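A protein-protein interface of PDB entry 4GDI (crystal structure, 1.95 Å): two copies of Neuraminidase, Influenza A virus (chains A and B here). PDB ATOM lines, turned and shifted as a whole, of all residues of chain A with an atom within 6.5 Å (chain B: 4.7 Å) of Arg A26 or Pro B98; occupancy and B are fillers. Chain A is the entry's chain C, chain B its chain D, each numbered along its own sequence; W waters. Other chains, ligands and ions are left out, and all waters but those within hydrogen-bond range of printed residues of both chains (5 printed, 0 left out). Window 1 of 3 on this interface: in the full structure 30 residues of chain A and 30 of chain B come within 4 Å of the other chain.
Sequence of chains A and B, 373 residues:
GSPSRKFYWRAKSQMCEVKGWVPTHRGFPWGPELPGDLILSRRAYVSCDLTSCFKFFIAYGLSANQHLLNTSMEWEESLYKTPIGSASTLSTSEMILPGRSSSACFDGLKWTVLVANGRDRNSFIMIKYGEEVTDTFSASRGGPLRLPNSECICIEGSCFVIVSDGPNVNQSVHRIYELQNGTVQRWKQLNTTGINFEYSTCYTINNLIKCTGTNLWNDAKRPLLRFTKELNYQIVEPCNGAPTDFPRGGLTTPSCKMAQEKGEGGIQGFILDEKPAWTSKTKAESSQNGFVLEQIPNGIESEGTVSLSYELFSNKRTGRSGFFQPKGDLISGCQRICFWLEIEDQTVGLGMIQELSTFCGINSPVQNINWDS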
ATOM      1  N   PRO A  23      25.607 -16.848 -21.355  1.00  0.00           N
ATOM      2  CA  PRO A  23      25.975 -18.259 -21.544  1.00  0.00           C
ATOM      3  C   PRO A  23      24.906 -19.029 -22.304  1.00  0.00           C
ATOM      4  O   PRO A  23      23.722 -18.958 -21.996  1.00  0.00           O
ATOM      5  CB  PRO A  23      26.093 -18.793 -20.117  1.00  0.00           C
ATOM      6  CG  PRO A  23      25.177 -17.900 -19.301  1.00  0.00           C
ATOM      7  CD  PRO A  23      25.185 -16.555 -19.971  1.00  0.00           C
ATOM      8  N   THR A  24      25.339 -19.761 -23.316  1.00  0.00           N
ATOM      9  CA  THR A  24      24.449 -20.591 -24.088  1.00  0.00           C
ATOM     10  C   THR A  24      24.664 -22.047 -23.688  1.00  0.00           C
ATOM     11  O   THR A  24      23.824 -22.890 -23.944  1.00  0.00           O
ATOM     12  CB  THR A  24      24.732 -20.416 -25.578  1.00  0.00           C
ATOM     13  OG1 THR A  24      26.140 -20.552 -25.797  1.00  0.00           O
ATOM     14  CG2 THR A  24      24.285 -19.032 -26.045  1.00  0.00           C
ATOM     15  N   HIS A  25      25.799 -22.319 -23.050  1.00  0.00           N
ATOM     16  CA  HIS A  25      26.137 -23.655 -22.573  1.00  0.00           C
ATOM     17  C   HIS A  25      27.107 -23.514 -21.409  1.00  0.00           C
ATOM     18  O   HIS A  25      28.214 -23.016 -21.574  1.00  0.00           O
ATOM     19  CB  HIS A  25      26.768 -24.467 -23.725  1.00  0.00           C
ATOM     20  CG  HIS A  25      27.433 -25.744 -23.300  1.00  0.00           C
ATOM     21  ND1 HIS A  25      26.781 -26.959 -23.293  1.00  0.00           N
ATOM     22  CD2 HIS A  25      28.704 -26.001 -22.906  1.00  0.00           C
ATOM     23  CE1 HIS A  25      27.615 -27.903 -22.894  1.00  0.00           C
ATOM     24  NE2 HIS A  25      28.789 -27.349 -22.657  1.00  0.00           N
ATOM     25  N   ARG A  26      26.686 -23.916 -20.218  1.00  0.00           N
ATOM     26  CA  ARG A  26      27.621 -24.054 -19.115  1.00  0.00           C
ATOM     27  C   ARG A  26      28.259 -25.409 -19.297  1.00  0.00           C
ATOM     28  O   ARG A  26      27.615 -26.332 -19.789  1.00  0.00           O
ATOM     29  CB  ARG A  26      26.911 -23.961 -17.762  1.00  0.00           C
ATOM     30  CG  ARG A  26      26.362 -22.581 -17.472  1.00  0.00           C
ATOM     31  CD  ARG A  26      25.662 -22.495 -16.121  1.00  0.00           C
ATOM     32  NE  ARG A  26      26.591 -22.284 -15.014  1.00  0.00           N
ATOM     33  CZ  ARG A  26      26.230 -21.888 -13.796  1.00  0.00           C
ATOM     34  NH1 ARG A  26      24.954 -21.653 -13.516  1.00  0.00           N
ATOM     35  NH2 ARG A  26      27.145 -21.728 -12.850  1.00  0.00           N
ATOM     36  N   GLY A  27      29.528 -25.535 -18.942  1.00  0.00           N
ATOM     37  CA  GLY A  27      30.177 -26.824 -19.053  1.00  0.00           C
ATOM     38  C   GLY A  27      29.410 -27.862 -18.256  1.00  0.00           C
ATOM     39  O   GLY A  27      28.682 -27.526 -17.325  1.00  0.00           O
ATOM     40  N   PHE A  28      29.554 -29.128 -18.616  1.00  0.00           N
ATOM     41  CA  PHE A  28      28.977 -30.179 -17.802  1.00  0.00           C
ATOM     42  C   PHE A  28      29.614 -30.109 -16.417  1.00  0.00           C
ATOM     43  O   PHE A  28      30.830 -29.990 -16.302  1.00  0.00           O
ATOM     44  CB  PHE A  28      29.166 -31.544 -18.461  1.00  0.00           C
ATOM     45  CG  PHE A  28      28.215 -31.782 -19.594  1.00  0.00           C
ATOM     46  CD1 PHE A  28      28.521 -31.344 -20.879  1.00  0.00           C
ATOM     47  CD2 PHE A  28      26.995 -32.401 -19.367  1.00  0.00           C
ATOM     48  CE1 PHE A  28      27.630 -31.534 -21.920  1.00  0.00           C
ATOM     49  CE2 PHE A  28      26.097 -32.595 -20.404  1.00  0.00           C
ATOM     50  CZ  PHE A  28      26.411 -32.152 -21.681  1.00  0.00           C
ATOM     51  N   PRO A  29      28.787 -30.169 -15.362  1.00  0.00           N
ATOM     52  CA  PRO A  29      29.211 -29.849 -13.997  1.00  0.00           C
ATOM     53  C   PRO A  29      29.922 -31.001 -13.298  1.00  0.00           C
ATOM     54  O   PRO A  29      29.615 -31.307 -12.145  1.00  0.00           O
ATOM     55  CB  PRO A  29      27.883 -29.538 -13.300  1.00  0.00           C
ATOM     56  CG  PRO A  29      26.900 -30.448 -13.983  1.00  0.00           C
ATOM     57  CD  PRO A  29      27.358 -30.539 -15.420  1.00  0.00           C
ATOM     58  N   PHE A 313      32.771 -14.508 -14.279  1.00  0.00           N
ATOM     59  CA  PHE A 313      33.169 -15.416 -13.205  1.00  0.00           C
ATOM     60  C   PHE A 313      34.073 -14.634 -12.270  1.00  0.00           C
ATOM     61  O   PHE A 313      34.793 -13.747 -12.718  1.00  0.00           O
ATOM     62  CB  PHE A 313      33.942 -16.629 -13.740  1.00  0.00           C
ATOM     63  CG  PHE A 313      33.131 -17.533 -14.626  1.00  0.00           C
ATOM     64  CD1 PHE A 313      32.270 -18.470 -14.081  1.00  0.00           C
ATOM     65  CD2 PHE A 313      33.241 -17.455 -16.006  1.00  0.00           C
ATOM     66  CE1 PHE A 313      31.523 -19.303 -14.897  1.00  0.00           C
ATOM     67  CE2 PHE A 313      32.495 -18.288 -16.823  1.00  0.00           C
ATOM     68  CZ  PHE A 313      31.636 -19.207 -16.271  1.00  0.00           C
ATOM     69  N   LYS A 316      35.710 -19.129  -9.955  1.00  0.00           N
ATOM     70  CA  LYS A 316      35.954 -20.343 -10.731  1.00  0.00           C
ATOM     71  C   LYS A 316      37.241 -20.219 -11.531  1.00  0.00           C
ATOM     72  O   LYS A 316      37.493 -19.185 -12.145  1.00  0.00           O
ATOM     73  CB  LYS A 316      34.789 -20.629 -11.670  1.00  0.00           C
ATOM     74  CG  LYS A 316      34.173 -21.996 -11.469  1.00  0.00           C
ATOM     75  CD  LYS A 316      32.827 -22.065 -12.149  1.00  0.00           C
ATOM     76  CE  LYS A 316      32.131 -23.376 -11.907  1.00  0.00           C
ATOM     77  NZ  LYS A 316      30.813 -23.368 -12.579  1.00  0.00           N
ATOM     78  N   GLU A 355      36.351 -28.228 -18.993  1.00  0.00           N
ATOM     79  CA  GLU A 355      35.062 -28.290 -19.685  1.00  0.00           C
ATOM     80  C   GLU A 355      34.796 -26.935 -20.317  1.00  0.00           C
ATOM     81  O   GLU A 355      35.025 -25.897 -19.693  1.00  0.00           O
ATOM     82  CB  GLU A 355      33.913 -28.626 -18.722  1.00  0.00           C
ATOM     83  CG  GLU A 355      33.711 -30.109 -18.467  1.00  0.00           C
ATOM     84  CD  GLU A 355      33.128 -30.827 -19.667  1.00  0.00           C
ATOM     85  OE1 GLU A 355      32.292 -30.218 -20.373  1.00  0.00           O
ATOM     86  OE2 GLU A 355      33.506 -31.995 -19.904  1.00  0.00           O
ATOM     87  N   LEU A 356      34.303 -26.943 -21.549  1.00  0.00           N
ATOM     88  CA  LEU A 356      34.025 -25.701 -22.250  1.00  0.00           C
ATOM     89  C   LEU A 356      32.660 -25.160 -21.880  1.00  0.00           C
ATOM     90  O   LEU A 356      31.674 -25.899 -21.877  1.00  0.00           O
ATOM     91  CB  LEU A 356      34.079 -25.915 -23.764  1.00  0.00           C
ATOM     92  CG  LEU A 356      35.453 -26.161 -24.388  1.00  0.00           C
ATOM     93  CD1 LEU A 356      35.335 -26.108 -25.891  1.00  0.00           C
ATOM     94  CD2 LEU A 356      36.483 -25.160 -23.895  1.00  0.00           C
ATOM     95  N   SER A 357      32.629 -23.877 -21.533  1.00  0.00           N
ATOM     96  CA  SER A 357      31.405 -23.069 -21.526  1.00  0.00           C
ATOM     97  C   SER A 357      31.373 -22.206 -22.798  1.00  0.00           C
ATOM     98  O   SER A 357      32.419 -21.889 -23.357  1.00  0.00           O
ATOM     99  CB  SER A 357      31.386 -22.148 -20.312  1.00  0.00           C
ATOM    100  OG  SER A 357      31.370 -22.897 -19.107  1.00  0.00           O
ATOM    101  N   THR A 358      30.187 -21.817 -23.253  1.00  0.00           N
ATOM    102  CA  THR A 358      30.091 -20.907 -24.393  1.00  0.00           C
ATOM    103  C   THR A 358      29.212 -19.699 -24.050  1.00  0.00           C
ATOM    104  O   THR A 358      28.149 -19.852 -23.445  1.00  0.00           O
ATOM    105  CB  THR A 358      29.517 -21.609 -25.638  1.00  0.00           C
ATOM    106  OG1 THR A 358      28.185 -22.060 -25.369  1.00  0.00           O
ATOM    107  CG2 THR A 358      30.394 -22.798 -26.071  1.00  0.00           C
ATOM    108  N   PHE A 359      29.673 -18.505 -24.430  1.00  0.00           N
ATOM    109  CA  PHE A 359      28.923 -17.271 -24.235  1.00  0.00           C
ATOM    110  C   PHE A 359      28.708 -16.595 -25.587  1.00  0.00           C
ATOM    111  O   PHE A 359      29.571 -16.667 -26.468  1.00  0.00           O
ATOM    112  CB  PHE A 359      29.685 -16.314 -23.320  1.00  0.00           C
ATOM    113  CG  PHE A 359      29.734 -16.740 -21.881  1.00  0.00           C
ATOM    114  CD1 PHE A 359      30.597 -17.733 -21.468  1.00  0.00           C
ATOM    115  CD2 PHE A 359      28.939 -16.109 -20.926  1.00  0.00           C
ATOM    116  CE1 PHE A 359      30.648 -18.122 -20.130  1.00  0.00           C
ATOM    117  CE2 PHE A 359      28.993 -16.489 -19.598  1.00  0.00           C
ATOM    118  CZ  PHE A 359      29.847 -17.501 -19.202  1.00  0.00           C
ATOM    119  N   ASN A 370      26.975 -12.990 -11.881  1.00  0.00           N
ATOM    120  CA  ASN A 370      28.169 -13.814 -11.724  1.00  0.00           C
ATOM    121  C   ASN A 370      27.779 -15.284 -11.800  1.00  0.00           C
ATOM    122  O   ASN A 370      26.928 -15.739 -11.037  1.00  0.00           O
ATOM    123  CB  ASN A 370      28.859 -13.534 -10.387  1.00  0.00           C
ATOM    124  CG  ASN A 370      30.039 -14.469 -10.125  1.00  0.00           C
ATOM    125  OD1 ASN A 370      30.151 -15.539 -10.722  1.00  0.00           O
ATOM    126  ND2 ASN A 370      30.919 -14.067  -9.218  1.00  0.00           N
ATOM    127  N   TRP A 371      28.421 -16.025 -12.703  1.00  0.00           N
ATOM    128  CA  TRP A 371      28.065 -17.422 -12.965  1.00  0.00           C
ATOM    129  C   TRP A 371      28.920 -18.461 -12.205  1.00  0.00           C
ATOM    130  O   TRP A 371      28.994 -19.620 -12.609  1.00  0.00           O
ATOM    131  CB  TRP A 371      28.144 -17.687 -14.470  1.00  0.00           C
ATOM    132  CG  TRP A 371      27.241 -16.799 -15.265  1.00  0.00           C
ATOM    133  CD1 TRP A 371      27.553 -15.589 -15.805  1.00  0.00           C
ATOM    134  CD2 TRP A 371      25.867 -17.043 -15.595  1.00  0.00           C
ATOM    135  NE1 TRP A 371      26.464 -15.067 -16.457  1.00  0.00           N
ATOM    136  CE2 TRP A 371      25.415 -15.938 -16.337  1.00  0.00           C
ATOM    137  CE3 TRP A 371      24.981 -18.090 -15.336  1.00  0.00           C
ATOM    138  CZ2 TRP A 371      24.114 -15.849 -16.825  1.00  0.00           C
ATOM    139  CZ3 TRP A 371      23.696 -18.002 -15.824  1.00  0.00           C
ATOM    140  CH2 TRP A 371      23.272 -16.891 -16.559  1.00  0.00           C
ATOM    141  N   ASP A 372      29.553 -18.061 -11.108  1.00  0.00           N
ATOM    142  CA  ASP A 372      30.398 -18.987 -10.349  1.00  0.00           C
ATOM    143  C   ASP A 372      29.606 -20.105  -9.668  1.00  0.00           C
ATOM    144  O   ASP A 372      29.975 -21.278  -9.748  1.00  0.00           O
ATOM    145  CB  ASP A 372      31.173 -18.246  -9.262  1.00  0.00           C
ATOM    146  CG  ASP A 372      32.327 -17.446  -9.803  1.00  0.00           C
ATOM    147  OD1 ASP A 372      32.985 -17.895 -10.761  1.00  0.00           O
ATOM    148  OD2 ASP A 372      32.589 -16.358  -9.251  1.00  0.00           O
ATOM    149  N   SER A 373      28.531 -19.740  -8.977  1.00  0.00           N
ATOM    150  CA  SER A 373      27.859 -20.689  -8.091  1.00  0.00           C
ATOM    151  C   SER A 373      26.449 -21.050  -8.570  1.00  0.00           C
ATOM    152  O   SER A 373      26.216 -21.262  -9.765  1.00  0.00           O
ATOM    153  CB  SER A 373      27.841 -20.149  -6.647  1.00  0.00           C
ATOM    154  OG  SER A 373      26.793 -19.220  -6.419  1.00  0.00           O
ATOM    155  OXT SER A 373      25.513 -21.163  -7.775  1.00  0.00           O
ATOM    156  N   GLU B  76      24.500 -25.847 -10.289  1.00  0.00           N
ATOM    157  CA  GLU B  76      24.667 -25.278 -11.625  1.00  0.00           C
ATOM    158  C   GLU B  76      23.566 -25.842 -12.514  1.00  0.00           C
ATOM    159  O   GLU B  76      23.705 -26.907 -13.120  1.00  0.00           O
ATOM    160  CB  GLU B  76      26.046 -25.601 -12.189  1.00  0.00           C
ATOM    161  CG  GLU B  76      27.158 -24.902 -11.430  1.00  0.00           C
ATOM    162  CD  GLU B  76      28.547 -25.386 -11.807  1.00  0.00           C
ATOM    163  OE1 GLU B  76      28.690 -26.125 -12.807  1.00  0.00           O
ATOM    164  OE2 GLU B  76      29.504 -25.016 -11.093  1.00  0.00           O
ATOM    165  N   GLU B  77      22.457 -25.118 -12.556  1.00  0.00           N
ATOM    166  CA  GLU B  77      21.219 -25.635 -13.123  1.00  0.00           C
ATOM    167  C   GLU B  77      21.138 -25.411 -14.624  1.00  0.00           C
ATOM    168  O   GLU B  77      21.358 -24.299 -15.106  1.00  0.00           O
ATOM    169  CB  GLU B  77      20.040 -24.960 -12.429  1.00  0.00           C
ATOM    170  CG  GLU B  77      20.116 -25.108 -10.922  1.00  0.00           C
ATOM    171  CD  GLU B  77      18.820 -24.780 -10.234  1.00  0.00           C
ATOM    172  OE1 GLU B  77      17.944 -25.664 -10.158  1.00  0.00           O
ATOM    173  OE2 GLU B  77      18.690 -23.642  -9.757  1.00  0.00           O
ATOM    174  N   SER B  78      20.820 -26.474 -15.356  1.00  0.00           N
ATOM    175  CA  SER B  78      20.599 -26.373 -16.795  1.00  0.00           C
ATOM    176  C   SER B  78      19.372 -27.151 -17.244  1.00  0.00           C
ATOM    177  O   SER B  78      19.010 -28.166 -16.650  1.00  0.00           O
ATOM    178  CB  SER B  78      21.821 -26.866 -17.561  1.00  0.00           C
ATOM    179  OG  SER B  78      22.950 -26.088 -17.227  1.00  0.00           O
ATOM    180  N   LEU B  79      18.744 -26.628 -18.297  1.00  0.00           N
ATOM    181  CA  LEU B  79      17.595 -27.221 -18.946  1.00  0.00           C
ATOM    182  C   LEU B  79      18.037 -28.301 -19.921  1.00  0.00           C
ATOM    183  O   LEU B  79      18.936 -28.087 -20.732  1.00  0.00           O
ATOM    184  CB  LEU B  79      16.827 -26.135 -19.708  1.00  0.00           C
ATOM    185  CG  LEU B  79      15.652 -26.610 -20.565  1.00  0.00           C
ATOM    186  CD1 LEU B  79      14.570 -27.234 -19.692  1.00  0.00           C
ATOM    187  CD2 LEU B  79      15.091 -25.473 -21.378  1.00  0.00           C
ATOM    188  N   MET B  95      21.534 -31.057 -23.514  1.00  0.00           N
ATOM    189  CA  MET B  95      21.570 -29.838 -22.721  1.00  0.00           C
ATOM    190  C   MET B  95      21.196 -28.664 -23.633  1.00  0.00           C
ATOM    191  O   MET B  95      21.803 -28.482 -24.676  1.00  0.00           O
ATOM    192  CB  MET B  95      22.963 -29.635 -22.115  1.00  0.00           C
ATOM    193  CG  MET B  95      23.063 -28.417 -21.212  1.00  0.00           C
ATOM    194  SD  MET B  95      24.757 -27.999 -20.741  1.00  0.00           S
ATOM    195  CE  MET B  95      25.029 -29.068 -19.333  1.00  0.00           C
ATOM    196  N   LEU B  97      20.060 -25.042 -22.435  1.00  0.00           N
ATOM    197  CA  LEU B  97      20.524 -23.752 -21.921  1.00  0.00           C
ATOM    198  C   LEU B  97      20.658 -23.839 -20.407  1.00  0.00           C
ATOM    199  O   LEU B  97      20.023 -24.677 -19.783  1.00  0.00           O
ATOM    200  CB  LEU B  97      19.498 -22.660 -22.219  1.00  0.00           C
ATOM    201  CG  LEU B  97      19.429 -22.098 -23.640  1.00  0.00           C
ATOM    202  CD1 LEU B  97      18.204 -21.210 -23.782  1.00  0.00           C
ATOM    203  CD2 LEU B  97      20.696 -21.319 -23.980  1.00  0.00           C
ATOM    204  N   PRO B  98      21.460 -22.960 -19.798  1.00  0.00           N
ATOM    205  CA  PRO B  98      21.374 -22.940 -18.331  1.00  0.00           C
ATOM    206  C   PRO B  98      20.073 -22.276 -17.902  1.00  0.00           C
ATOM    207  O   PRO B  98      19.551 -21.435 -18.626  1.00  0.00           O
ATOM    208  CB  PRO B  98      22.599 -22.122 -17.908  1.00  0.00           C
ATOM    209  CG  PRO B  98      22.931 -21.276 -19.097  1.00  0.00           C
ATOM    210  CD  PRO B  98      22.465 -22.023 -20.328  1.00  0.00           C
ATOM    211  N   GLY B  99      19.526 -22.657 -16.758  1.00  0.00           N
ATOM    212  CA  GLY B  99      18.270 -22.081 -16.330  1.00  0.00           C
ATOM    213  C   GLY B  99      17.734 -22.700 -15.054  1.00  0.00           C
ATOM    214  O   GLY B  99      17.909 -23.895 -14.838  1.00  0.00           O
ATOM    215  N   VAL B 115      14.410 -19.503 -20.708  1.00  0.00           N
ATOM    216  CA  VAL B 115      14.942 -19.857 -19.380  1.00  0.00           C
ATOM    217  C   VAL B 115      15.162 -18.606 -18.551  1.00  0.00           C
ATOM    218  O   VAL B 115      15.419 -17.539 -19.098  1.00  0.00           O
ATOM    219  CB  VAL B 115      16.299 -20.577 -19.444  1.00  0.00           C
ATOM    220  CG1 VAL B 115      16.159 -21.957 -20.101  1.00  0.00           C
ATOM    221  CG2 VAL B 115      17.333 -19.713 -20.162  1.00  0.00           C
ATOM    222  N   ASN B 117      17.468 -17.010 -15.285  1.00  0.00           N
ATOM    223  CA  ASN B 117      18.697 -17.176 -14.523  1.00  0.00           C
ATOM    224  C   ASN B 117      18.934 -15.950 -13.667  1.00  0.00           C
ATOM    225  O   ASN B 117      18.437 -14.862 -13.979  1.00  0.00           O
ATOM    226  CB  ASN B 117      19.908 -17.362 -15.433  1.00  0.00           C
ATOM    227  CG  ASN B 117      19.936 -18.715 -16.109  1.00  0.00           C
ATOM    228  OD1 ASN B 117      20.398 -19.711 -15.539  1.00  0.00           O
ATOM    229  ND2 ASN B 117      19.448 -18.757 -17.340  1.00  0.00           N
ATOM    230  N   MET B 126      16.116 -15.398 -21.052  1.00  0.00           N
ATOM    231  CA  MET B 126      16.802 -15.543 -22.331  1.00  0.00           C
ATOM    232  C   MET B 126      15.902 -16.400 -23.197  1.00  0.00           C
ATOM    233  O   MET B 126      15.264 -17.322 -22.697  1.00  0.00           O
ATOM    234  CB  MET B 126      18.100 -16.285 -22.096  1.00  0.00           C
ATOM    235  CG  MET B 126      19.233 -15.955 -23.022  1.00  0.00           C
ATOM    236  SD  MET B 126      20.699 -16.924 -22.598  1.00  0.00           S
ATOM    237  CE  MET B 126      20.347 -17.435 -20.921  1.00  0.00           C
HETATM  238  O   HOH W   1      23.904 -25.050 -19.882  1.00  0.00           O
HETATM  239  O   HOH W   2      22.230 -21.786 -14.563  1.00  0.00           O
HETATM  240  O   HOH W   3      27.336 -26.260 -15.374  1.00  0.00           O
HETATM  241  O   HOH W   4      22.302 -22.316 -11.560  1.00  0.00           O
HETATM  242  O   HOH W   5      24.340 -26.796 -24.562  1.00  0.00           O
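A ring nitrogen (ND1) of His A25 lies within hydrogen-bond range of the side-chain sulfur of Met B95 (3.4 Å).
The side-chain amino group (NZ) of Lys A316 is in salt-bridge range of the side-chain carboxylate (OE2) of Glu B76, 2.6 Å away.
The side-chain sulfur of Met B126 sits close to the backbone carbonyl oxygen of Pro A23 (3.7 Å).
The backbone carbonyl oxygen of Arg A26 lies close to the side-chain sulfur of Met B95, at 3.4 Å.
Among the printed residues, merely in contact across the chains: Pro A23 with Pro B98 (3.7 Å), Thr A24 with Leu B97 (3.5 Å), Thr A24 with Pro B98 (3.96 Å), Arg A26 with Glu B76 (3.5 Å), Arg A26 with Pro B98 (3.6 Å), Phe A28 with Met B95 (3.8 Å), Pro A29 with Glu B76 (3.5 Å) and Trp A371 with Asn B117 (3.6 Å).
Of the printed residues of chain B, Thr A24 touches Leu B97 (3.5 Å) and Pro B98 (3.96 Å).
Arg A26 touches just these residues of chain B: Glu B76, Met B95 and Pro B98.
Printed residues of chain B within 4 Å of Trp A371: Asn B117.
Ser A373 touches none of the printed residues of chain B.
Printed residues of chain A within 4 Å of Glu B76: Arg A26, Pro A29 and Lys A316.
Printed residues of chain A within 4 Å of Leu B97: Thr A24.
Of the printed residues of chain A, Pro B98 touches Pro A23 (3.7 Å), Thr A24 (3.96 Å) and Arg A26 (3.6 Å).
The nearest residue of chain B that does not touch Arg A26 is Glu B77 (4.4 Å).
The nearest printed residue of chain A that does not touch Leu B97 is Pro A23 (4.3 Å).
Of the 11 printed residues of chain B, 6 touch a printed residue of chain A.
Hydrophobic or aromatic side chains of chain B within 4 Å of the printed part of chain A: Met B95, Leu B97, Pro B98 and Met B126.
Printed residues of chain A that touch a printed residue of chain B: Pro A23, Thr A24, His A25, Arg A26, Phe A28, Pro A29, Lys A316 and Trp A371.
Among the printed residues, 12 pairs touch across the chains.
Among the printed residues, Asp or Glu carboxylates within 4 Å of a Lys or Arg side-chain nitrogen of the other chain: Lys A316 with Glu B76 (2.6 Å).
No position is printed for both chains.
Water W3 bridges O of Gly A27 (2.7 Å) and OE1 of Glu B76 (2.9 Å).
Water W2 lies within hydrogen-bond range of the backbone carbonyl oxygen of Glu B77, the guanidinium group of Arg A26 and the side-chain amide oxygen of Asn B117.
Water W5 lies within hydrogen-bond range of a ring nitrogen (ND1) of His A25 and the backbone carbonyl oxygen of Met B95.
Water W4 lies within hydrogen-bond range of the backbone NH (N) of Glu B77 (3.0 Å) and the guanidinium group (NH1) of Arg A26 (3.4 Å).
Water W1 lies within hydrogen-bond range of OG of Ser B78 (3.0 Å), N of Arg A26 (3.0 Å) and SD of Met B95 (3.2 Å).
N of Gly B99 lies close to OD1 of Asn B117, at 3.3 Å.
NH2 of Arg A26 lies within salt-bridge range of O of Ser A373 (3.3 Å).
The guanidinium group (NH2) of Arg A26 is in hydrogen-bond range of the backbone carbonyl oxygen (O) of Trp A371 (2.8 Å).
The backbone NH of Lys A316 lies within hydrogen-bond range of the side-chain carboxylate of Asp A372 (3.1 Å).
N of Phe A28 is in hydrogen-bond range of OE1 of Glu A355 (3.4 Å).
The side-chain hydroxyl (OG1) of Thr A358 is in hydrogen-bond range of the side-chain hydroxyl (OG1) of Thr A24 (2.6 Å).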
